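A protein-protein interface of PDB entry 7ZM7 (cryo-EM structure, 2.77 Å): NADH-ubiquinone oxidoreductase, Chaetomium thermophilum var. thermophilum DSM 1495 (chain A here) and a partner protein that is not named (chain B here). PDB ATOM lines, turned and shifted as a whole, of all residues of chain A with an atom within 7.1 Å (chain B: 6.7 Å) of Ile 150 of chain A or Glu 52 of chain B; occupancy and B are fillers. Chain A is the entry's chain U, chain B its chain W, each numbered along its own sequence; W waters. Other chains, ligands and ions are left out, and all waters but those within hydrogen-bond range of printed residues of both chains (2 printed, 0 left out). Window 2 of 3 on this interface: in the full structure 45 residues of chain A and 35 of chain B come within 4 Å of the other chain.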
ATOM      1  N   TRP A 110     -30.493  14.545  17.770  1.00  0.00           N
ATOM      2  CA  TRP A 110     -29.477  15.039  18.727  1.00  0.00           C
ATOM      3  C   TRP A 110     -29.401  16.567  18.672  1.00  0.00           C
ATOM      4  O   TRP A 110     -28.732  17.154  19.536  1.00  0.00           O
ATOM      5  CB  TRP A 110     -28.128  14.376  18.438  1.00  0.00           C
ATOM      6  CG  TRP A 110     -27.571  14.579  17.064  1.00  0.00           C
ATOM      7  CD1 TRP A 110     -26.732  15.573  16.657  1.00  0.00           C
ATOM      8  CD2 TRP A 110     -27.760  13.725  15.922  1.00  0.00           C
ATOM      9  NE1 TRP A 110     -26.409  15.411  15.337  1.00  0.00           N
ATOM     10  CE2 TRP A 110     -27.021  14.286  14.861  1.00  0.00           C
ATOM     11  CE3 TRP A 110     -28.490  12.556  15.689  1.00  0.00           C
ATOM     12  CZ2 TRP A 110     -26.985  13.709  13.594  1.00  0.00           C
ATOM     13  CZ3 TRP A 110     -28.456  11.988  14.436  1.00  0.00           C
ATOM     14  CH2 TRP A 110     -27.718  12.561  13.403  1.00  0.00           C
ATOM     15  N   ARG A 113     -32.332  18.404  21.679  1.00  0.00           N
ATOM     16  CA  ARG A 113     -32.562  17.717  22.945  1.00  0.00           C
ATOM     17  C   ARG A 113     -33.362  18.537  23.941  1.00  0.00           C
ATOM     18  O   ARG A 113     -34.273  17.968  24.560  1.00  0.00           O
ATOM     19  CB  ARG A 113     -31.228  17.271  23.543  1.00  0.00           C
ATOM     20  CG  ARG A 113     -30.508  16.279  22.691  1.00  0.00           C
ATOM     21  CD  ARG A 113     -31.255  14.993  22.550  1.00  0.00           C
ATOM     22  NE  ARG A 113     -30.361  13.982  22.009  1.00  0.00           N
ATOM     23  CZ  ARG A 113     -30.751  12.854  21.437  1.00  0.00           C
ATOM     24  NH1 ARG A 113     -29.854  12.014  20.968  1.00  0.00           N
ATOM     25  NH2 ARG A 113     -32.030  12.564  21.327  1.00  0.00           N
ATOM     26  N   VAL A 143     -27.599   7.576  24.803  1.00  0.00           N
ATOM     27  CA  VAL A 143     -27.225   8.750  23.972  1.00  0.00           C
ATOM     28  C   VAL A 143     -28.336   9.802  24.033  1.00  0.00           C
ATOM     29  O   VAL A 143     -28.010  10.988  24.016  1.00  0.00           O
ATOM     30  CB  VAL A 143     -26.864   8.303  22.538  1.00  0.00           C
ATOM     31  CG1 VAL A 143     -28.082   8.065  21.659  1.00  0.00           C
ATOM     32  CG2 VAL A 143     -25.895   9.267  21.871  1.00  0.00           C
ATOM     33  N   ARG A 146     -27.885  12.042  27.289  1.00  0.00           N
ATOM     34  CA  ARG A 146     -26.619  12.642  27.685  1.00  0.00           C
ATOM     35  C   ARG A 146     -26.718  14.151  27.748  1.00  0.00           C
ATOM     36  O   ARG A 146     -27.270  14.790  26.856  1.00  0.00           O
ATOM     37  CB  ARG A 146     -25.512  12.271  26.710  1.00  0.00           C
ATOM     38  CG  ARG A 146     -25.040  10.888  26.853  1.00  0.00           C
ATOM     39  CD  ARG A 146     -24.371  10.387  25.633  1.00  0.00           C
ATOM     40  NE  ARG A 146     -24.089   8.968  25.769  1.00  0.00           N
ATOM     41  CZ  ARG A 146     -22.974   8.386  25.364  1.00  0.00           C
ATOM     42  NH1 ARG A 146     -22.823   7.087  25.523  1.00  0.00           N
ATOM     43  NH2 ARG A 146     -22.016   9.097  24.804  1.00  0.00           N
ATOM     44  N   ARG A 148     -24.370  16.149  27.267  1.00  0.00           N
ATOM     45  CA  ARG A 148     -23.620  16.728  26.135  1.00  0.00           C
ATOM     46  C   ARG A 148     -23.872  15.927  24.857  1.00  0.00           C
ATOM     47  O   ARG A 148     -23.874  14.692  24.928  1.00  0.00           O
ATOM     48  CB  ARG A 148     -22.133  16.741  26.485  1.00  0.00           C
ATOM     49  CG  ARG A 148     -21.832  17.294  27.871  1.00  0.00           C
ATOM     50  CD  ARG A 148     -20.370  17.647  28.064  1.00  0.00           C
ATOM     51  NE  ARG A 148     -20.010  18.878  27.373  1.00  0.00           N
ATOM     52  CZ  ARG A 148     -20.022  20.084  27.930  1.00  0.00           C
ATOM     53  NH1 ARG A 148     -19.679  21.144  27.218  1.00  0.00           N
ATOM     54  NH2 ARG A 148     -20.371  20.227  29.196  1.00  0.00           N
ATOM     55  N   GLN A 149     -24.153  16.607  23.746  1.00  0.00           N
ATOM     56  CA  GLN A 149     -24.251  15.900  22.448  1.00  0.00           C
ATOM     57  C   GLN A 149     -23.091  16.407  21.609  1.00  0.00           C
ATOM     58  O   GLN A 149     -23.052  17.605  21.323  1.00  0.00           O
ATOM     59  CB  GLN A 149     -25.600  16.142  21.765  1.00  0.00           C
ATOM     60  CG  GLN A 149     -26.791  15.527  22.483  1.00  0.00           C
ATOM     61  CD  GLN A 149     -26.745  14.022  22.582  1.00  0.00           C
ATOM     62  OE1 GLN A 149     -26.355  13.325  21.651  1.00  0.00           O
ATOM     63  NE2 GLN A 149     -27.168  13.508  23.724  1.00  0.00           N
ATOM     64  N   ILE A 150     -22.162  15.515  21.281  1.00  0.00           N
ATOM     65  CA  ILE A 150     -20.931  15.911  20.547  1.00  0.00           C
ATOM     66  C   ILE A 150     -21.314  16.429  19.165  1.00  0.00           C
ATOM     67  O   ILE A 150     -20.749  17.442  18.742  1.00  0.00           O
ATOM     68  CB  ILE A 150     -20.018  14.672  20.439  1.00  0.00           C
ATOM     69  CG1 ILE A 150     -19.424  14.263  21.788  1.00  0.00           C
ATOM     70  CG2 ILE A 150     -18.946  14.847  19.376  1.00  0.00           C
ATOM     71  CD1 ILE A 150     -18.761  12.905  21.773  1.00  0.00           C
ATOM     72  N   PHE A 151     -22.251  15.756  18.498  1.00  0.00           N
ATOM     73  CA  PHE A 151     -22.540  16.104  17.092  1.00  0.00           C
ATOM     74  C   PHE A 151     -23.599  17.195  16.981  1.00  0.00           C
ATOM     75  O   PHE A 151     -23.966  17.536  15.849  1.00  0.00           O
ATOM     76  CB  PHE A 151     -22.768  14.828  16.286  1.00  0.00           C
ATOM     77  CG  PHE A 151     -21.593  13.886  16.274  1.00  0.00           C
ATOM     78  CD1 PHE A 151     -20.525  14.097  15.419  1.00  0.00           C
ATOM     79  CD2 PHE A 151     -21.550  12.795  17.126  1.00  0.00           C
ATOM     80  CE1 PHE A 151     -19.441  13.237  15.413  1.00  0.00           C
ATOM     81  CE2 PHE A 151     -20.466  11.935  17.120  1.00  0.00           C
ATOM     82  CZ  PHE A 151     -19.415  12.157  16.263  1.00  0.00           C
ATOM     83  N   ALA A 152     -24.048  17.744  18.114  1.00  0.00           N
ATOM     84  CA  ALA A 152     -24.991  18.888  18.075  1.00  0.00           C
ATOM     85  C   ALA A 152     -24.281  20.116  17.505  1.00  0.00           C
ATOM     86  O   ALA A 152     -23.108  20.317  17.829  1.00  0.00           O
ATOM     87  CB  ALA A 152     -25.539  19.166  19.441  1.00  0.00           C
ATOM     88  N   HIS A 153     -24.983  20.916  16.703  1.00  0.00           N
ATOM     89  CA  HIS A 153     -24.379  22.106  16.050  1.00  0.00           C
ATOM     90  C   HIS A 153     -24.363  23.229  17.067  1.00  0.00           C
ATOM     91  O   HIS A 153     -23.416  24.024  17.050  1.00  0.00           O
ATOM     92  CB  HIS A 153     -25.235  22.526  14.859  1.00  0.00           C
ATOM     93  CG  HIS A 153     -25.130  21.629  13.675  1.00  0.00           C
ATOM     94  ND1 HIS A 153     -25.556  22.015  12.426  1.00  0.00           N
ATOM     95  CD2 HIS A 153     -24.647  20.378  13.541  1.00  0.00           C
ATOM     96  CE1 HIS A 153     -25.343  21.038  11.573  1.00  0.00           C
ATOM     97  NE2 HIS A 153     -24.793  20.023  12.231  1.00  0.00           N
ATOM     98  N   ILE A 156     -25.838  22.192  24.170  1.00  0.00           N
ATOM     99  CA  ILE A 156     -27.021  22.038  25.061  1.00  0.00           C
ATOM    100  C   ILE A 156     -26.736  22.823  26.348  1.00  0.00           C
ATOM    101  O   ILE A 156     -25.745  22.480  27.005  1.00  0.00           O
ATOM    102  CB  ILE A 156     -27.355  20.567  25.350  1.00  0.00           C
ATOM    103  CG1 ILE A 156     -27.578  19.763  24.070  1.00  0.00           C
ATOM    104  CG2 ILE A 156     -28.539  20.462  26.297  1.00  0.00           C
ATOM    105  CD1 ILE A 156     -27.774  18.297  24.323  1.00  0.00           C
ATOM    106  N   LYS B  45     -10.220  10.941  21.590  1.00  0.00           N
ATOM    107  CA  LYS B  45     -11.392  11.765  21.191  1.00  0.00           C
ATOM    108  C   LYS B  45     -12.172  11.087  20.061  1.00  0.00           C
ATOM    109  O   LYS B  45     -13.402  11.130  20.108  1.00  0.00           O
ATOM    110  CB  LYS B  45     -10.921  13.194  20.904  1.00  0.00           C
ATOM    111  CG  LYS B  45     -10.147  13.858  22.029  1.00  0.00           C
ATOM    112  CD  LYS B  45     -11.013  14.104  23.233  1.00  0.00           C
ATOM    113  CE  LYS B  45     -12.221  14.956  22.910  1.00  0.00           C
ATOM    114  NZ  LYS B  45     -13.258  14.843  23.960  1.00  0.00           N
ATOM    115  N   VAL B  47     -12.267   7.802  19.488  1.00  0.00           N
ATOM    116  CA  VAL B  47     -12.873   6.528  19.971  1.00  0.00           C
ATOM    117  C   VAL B  47     -14.134   6.845  20.765  1.00  0.00           C
ATOM    118  O   VAL B  47     -15.036   6.011  20.809  1.00  0.00           O
ATOM    119  CB  VAL B  47     -11.868   5.644  20.751  1.00  0.00           C
ATOM    120  CG1 VAL B  47     -12.517   4.694  21.743  1.00  0.00           C
ATOM    121  CG2 VAL B  47     -10.918   4.894  19.835  1.00  0.00           C
ATOM    122  N   LYS B  48     -14.240   8.065  21.261  1.00  0.00           N
ATOM    123  CA  LYS B  48     -15.453   8.459  22.013  1.00  0.00           C
ATOM    124  C   LYS B  48     -16.514   8.911  21.012  1.00  0.00           C
ATOM    125  O   LYS B  48     -17.681   8.555  21.197  1.00  0.00           O
ATOM    126  CB  LYS B  48     -15.137   9.590  22.992  1.00  0.00           C
ATOM    127  CG  LYS B  48     -14.240   9.240  24.165  1.00  0.00           C
ATOM    128  CD  LYS B  48     -14.501  10.127  25.355  1.00  0.00           C
ATOM    129  CE  LYS B  48     -15.918  10.006  25.872  1.00  0.00           C
ATOM    130  NZ  LYS B  48     -16.166  10.920  27.012  1.00  0.00           N
ATOM    131  N   GLY B  49     -16.108   9.656  19.986  1.00  0.00           N
ATOM    132  CA  GLY B  49     -17.055  10.188  18.998  1.00  0.00           C
ATOM    133  C   GLY B  49     -17.713   9.119  18.158  1.00  0.00           C
ATOM    134  O   GLY B  49     -18.930   9.193  17.956  1.00  0.00           O
ATOM    135  N   ILE B  50     -16.941   8.161  17.660  1.00  0.00           N
ATOM    136  CA  ILE B  50     -17.558   7.178  16.736  1.00  0.00           C
ATOM    137  C   ILE B  50     -18.442   6.228  17.554  1.00  0.00           C
ATOM    138  O   ILE B  50     -19.337   5.623  16.981  1.00  0.00           O
ATOM    139  CB  ILE B  50     -16.460   6.458  15.931  1.00  0.00           C
ATOM    140  CG1 ILE B  50     -15.562   7.450  15.192  1.00  0.00           C
ATOM    141  CG2 ILE B  50     -17.057   5.440  14.973  1.00  0.00           C
ATOM    142  CD1 ILE B  50     -14.510   6.790  14.333  1.00  0.00           C
ATOM    143  N   ARG B  51     -18.215   6.136  18.859  1.00  0.00           N
ATOM    144  CA  ARG B  51     -19.101   5.321  19.726  1.00  0.00           C
ATOM    145  C   ARG B  51     -20.442   6.054  19.809  1.00  0.00           C
ATOM    146  O   ARG B  51     -21.484   5.415  19.620  1.00  0.00           O
ATOM    147  CB  ARG B  51     -18.362   4.926  21.003  1.00  0.00           C
ATOM    148  CG  ARG B  51     -17.401   3.759  20.833  1.00  0.00           C
ATOM    149  CD  ARG B  51     -17.349   2.921  22.092  1.00  0.00           C
ATOM    150  NE  ARG B  51     -16.495   1.749  21.983  1.00  0.00           N
ATOM    151  CZ  ARG B  51     -15.331   1.610  22.604  1.00  0.00           C
ATOM    152  NH1 ARG B  51     -14.626   0.503  22.452  1.00  0.00           N
ATOM    153  NH2 ARG B  51     -14.883   2.569  23.392  1.00  0.00           N
ATOM    154  N   GLU B  52     -20.394   7.358  20.099  1.00  0.00           N
ATOM    155  CA  GLU B  52     -21.616   8.203  20.161  1.00  0.00           C
ATOM    156  C   GLU B  52     -22.315   8.238  18.799  1.00  0.00           C
ATOM    157  O   GLU B  52     -23.552   8.175  18.785  1.00  0.00           O
ATOM    158  CB  GLU B  52     -21.261   9.609  20.647  1.00  0.00           C
ATOM    159  CG  GLU B  52     -22.372  10.630  20.493  1.00  0.00           C
ATOM    160  CD  GLU B  52     -22.455  11.668  21.599  1.00  0.00           C
ATOM    161  OE1 GLU B  52     -21.964  11.392  22.714  1.00  0.00           O
ATOM    162  OE2 GLU B  52     -23.016  12.751  21.345  1.00  0.00           O
ATOM    163  N   GLN B  53     -21.560   8.307  17.706  1.00  0.00           N
ATOM    164  CA  GLN B  53     -22.167   8.340  16.357  1.00  0.00           C
ATOM    165  C   GLN B  53     -22.961   7.057  16.154  1.00  0.00           C
ATOM    166  O   GLN B  53     -24.091   7.134  15.677  1.00  0.00           O
ATOM    167  CB  GLN B  53     -21.091   8.348  15.277  1.00  0.00           C
ATOM    168  CG  GLN B  53     -21.083   9.591  14.409  1.00  0.00           C
ATOM    169  CD  GLN B  53     -19.937   9.525  13.432  1.00  0.00           C
ATOM    170  OE1 GLN B  53     -19.381   8.462  13.179  1.00  0.00           O
ATOM    171  NE2 GLN B  53     -19.576  10.666  12.871  1.00  0.00           N
ATOM    172  N   ASN B  54     -22.395   5.926  16.542  1.00  0.00           N
ATOM    173  CA  ASN B  54     -23.049   4.608  16.364  1.00  0.00           C
ATOM    174  C   ASN B  54     -24.333   4.552  17.191  1.00  0.00           C
ATOM    175  O   ASN B  54     -25.297   3.952  16.720  1.00  0.00           O
ATOM    176  CB  ASN B  54     -22.041   3.498  16.643  1.00  0.00           C
ATOM    177  CG  ASN B  54     -21.043   3.304  15.524  1.00  0.00           C
ATOM    178  OD1 ASN B  54     -21.293   3.696  14.391  1.00  0.00           O
ATOM    179  ND2 ASN B  54     -19.913   2.687  15.824  1.00  0.00           N
ATOM    180  N   GLU B  55     -24.318   5.115  18.392  1.00  0.00           N
ATOM    181  CA  GLU B  55     -25.517   5.175  19.267  1.00  0.00           C
ATOM    182  C   GLU B  55     -26.584   6.115  18.689  1.00  0.00           C
ATOM    183  O   GLU B  55     -27.781   5.824  18.850  1.00  0.00           O
ATOM    184  CB  GLU B  55     -25.074   5.409  20.712  1.00  0.00           C
ATOM    185  CG  GLU B  55     -24.325   4.231  21.297  1.00  0.00           C
ATOM    186  CD  GLU B  55     -24.871   2.879  20.872  1.00  0.00           C
ATOM    187  OE1 GLU B  55     -26.094   2.662  21.003  1.00  0.00           O
ATOM    188  OE2 GLU B  55     -24.071   2.044  20.406  1.00  0.00           O
ATOM    189  N   LEU B  56     -26.175   7.222  18.073  1.00  0.00           N
ATOM    190  CA  LEU B  56     -27.144   8.121  17.394  1.00  0.00           C
ATOM    191  C   LEU B  56     -27.793   7.364  16.239  1.00  0.00           C
ATOM    192  O   LEU B  56     -28.989   7.552  16.011  1.00  0.00           O
ATOM    193  CB  LEU B  56     -26.434   9.393  16.928  1.00  0.00           C
ATOM    194  CG  LEU B  56     -25.987  10.340  18.035  1.00  0.00           C
ATOM    195  CD1 LEU B  56     -25.123  11.455  17.472  1.00  0.00           C
ATOM    196  CD2 LEU B  56     -27.186  10.903  18.774  1.00  0.00           C
ATOM    197  N   ALA B  57     -27.022   6.542  15.538  1.00  0.00           N
ATOM    198  CA  ALA B  57     -27.572   5.708  14.450  1.00  0.00           C
ATOM    199  C   ALA B  57     -28.595   4.681  14.966  1.00  0.00           C
ATOM    200  O   ALA B  57     -29.573   4.439  14.257  1.00  0.00           O
ATOM    201  CB  ALA B  57     -26.463   5.090  13.644  1.00  0.00           C
HETATM  202  O   HOH W   1     -18.867   8.973  23.737  1.00  0.00           O
HETATM  203  O   HOH W   2     -24.222  14.259  19.336  1.00  0.00           O
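The side-chain carboxylate (OE1) of Glu 52 of chain B lies within salt-bridge range of the guanidinium group (NH2) of Arg 146 of chain A, 3.1 Å away. The side-chain carboxylate of Glu 52 of chain B lies within hydrogen-bond range of the backbone NH of Ile 150 of chain A. The side-chain amide oxygen (OE1) of Gln 149 of chain A sits close to the side-chain carboxylate (OE2) of Glu 52 of chain B, at 3.4 Å.
The indole nitrogen (NE1) of Trp 110 of chain A is in hydrogen-bond range of the backbone carbonyl oxygen (O) of Phe 151 of chain A. O of Val 143 of chain A lies within hydrogen-bond range of NE2 of Gln 149 of chain A (2.7 Å). O of Arg 146 of chain A is in hydrogen-bond range of NE2 of Gln 149 of chain A, 3.4 Å away.
Trp 110 of chain A touches Leu 56 of chain B (CB to CD2, 3.6 Å). Leu 56 of chain B touches Arg 113 of chain A. Val 143 of chain A touches Glu 55 of chain B (CG1 to O, 3.6 Å). Leu 56 of chain B touches Val 143 of chain A (CD2 to CG2, 3.7 Å). Leu 56 of chain B touches Gln 149 of chain A (CD2 to OE1, 3.9 Å). Phe 151 of chain A touches Gly 49 of chain B. Phe 151 of chain A touches Gln 53 of chain B (CZ to CG, 3.6 Å). Phe 151 of chain A touches Leu 56 of chain B.
Ile 150 of chain A touches one residue of chain B. Of the printed residues of chain A, Glu 52 of chain B touches Arg 146 (3.1 Å), Gln 149 (3.4 Å) and Ile 150 (2.9 Å). Of the printed residues of chain B, Trp 110 of chain A touches Leu 56 (3.6 Å). Of the printed residues of chain A, Gln 53 of chain B touches Phe 151 (3.6 Å). Of the printed residues of chain A, Gly 49 of chain B touches Phe 151. Of the printed residues of chain B, Arg 146 of chain A touches Glu 52 (3.1 Å). His 153 of chain A touches none of the printed residues of chain B. The nearest residue of chain B that does not touch Ile 150 of chain A is Gly 49 of chain B (4.2 Å). The nearest residue of chain A that does not touch Glu 52 of chain B is Val 143 of chain A (4.02 Å).
Of the 11 printed residues of chain A, 7 touch a printed residue of chain B. Hydrophobic or aromatic side chains of chain A within 4 Å of the printed part of chain B: Trp 110, Val 143, Ile 150 and Phe 151. Of the 12 printed residues of chain B, 5 touch a printed residue of chain A. Hydrophobic or aromatic side chains of chain B that line the printed part of chain A: Leu 56. Among the printed residues, Asp or Glu carboxylates within 4 Å of a Lys or Arg side-chain nitrogen of the other chain: Arg 146 of chain A with Glu 52 of chain B (3.1 Å).
Water W2 lies within hydrogen-bond range of the backbone NH (N) of Phe 151 of chain A (2.6 Å), the side-chain carboxylate (OE2) of Glu 52 of chain B (2.8 Å), the backbone NH (N) of Ile 150 of chain A (3.1 Å) and the side-chain amide oxygen (OE1) of Gln 149 of chain A (3.3 Å). Water W1 bridges the backbone carbonyl oxygen of Lys 48 of chain B and the guanidinium group of Arg 146 of chain A.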
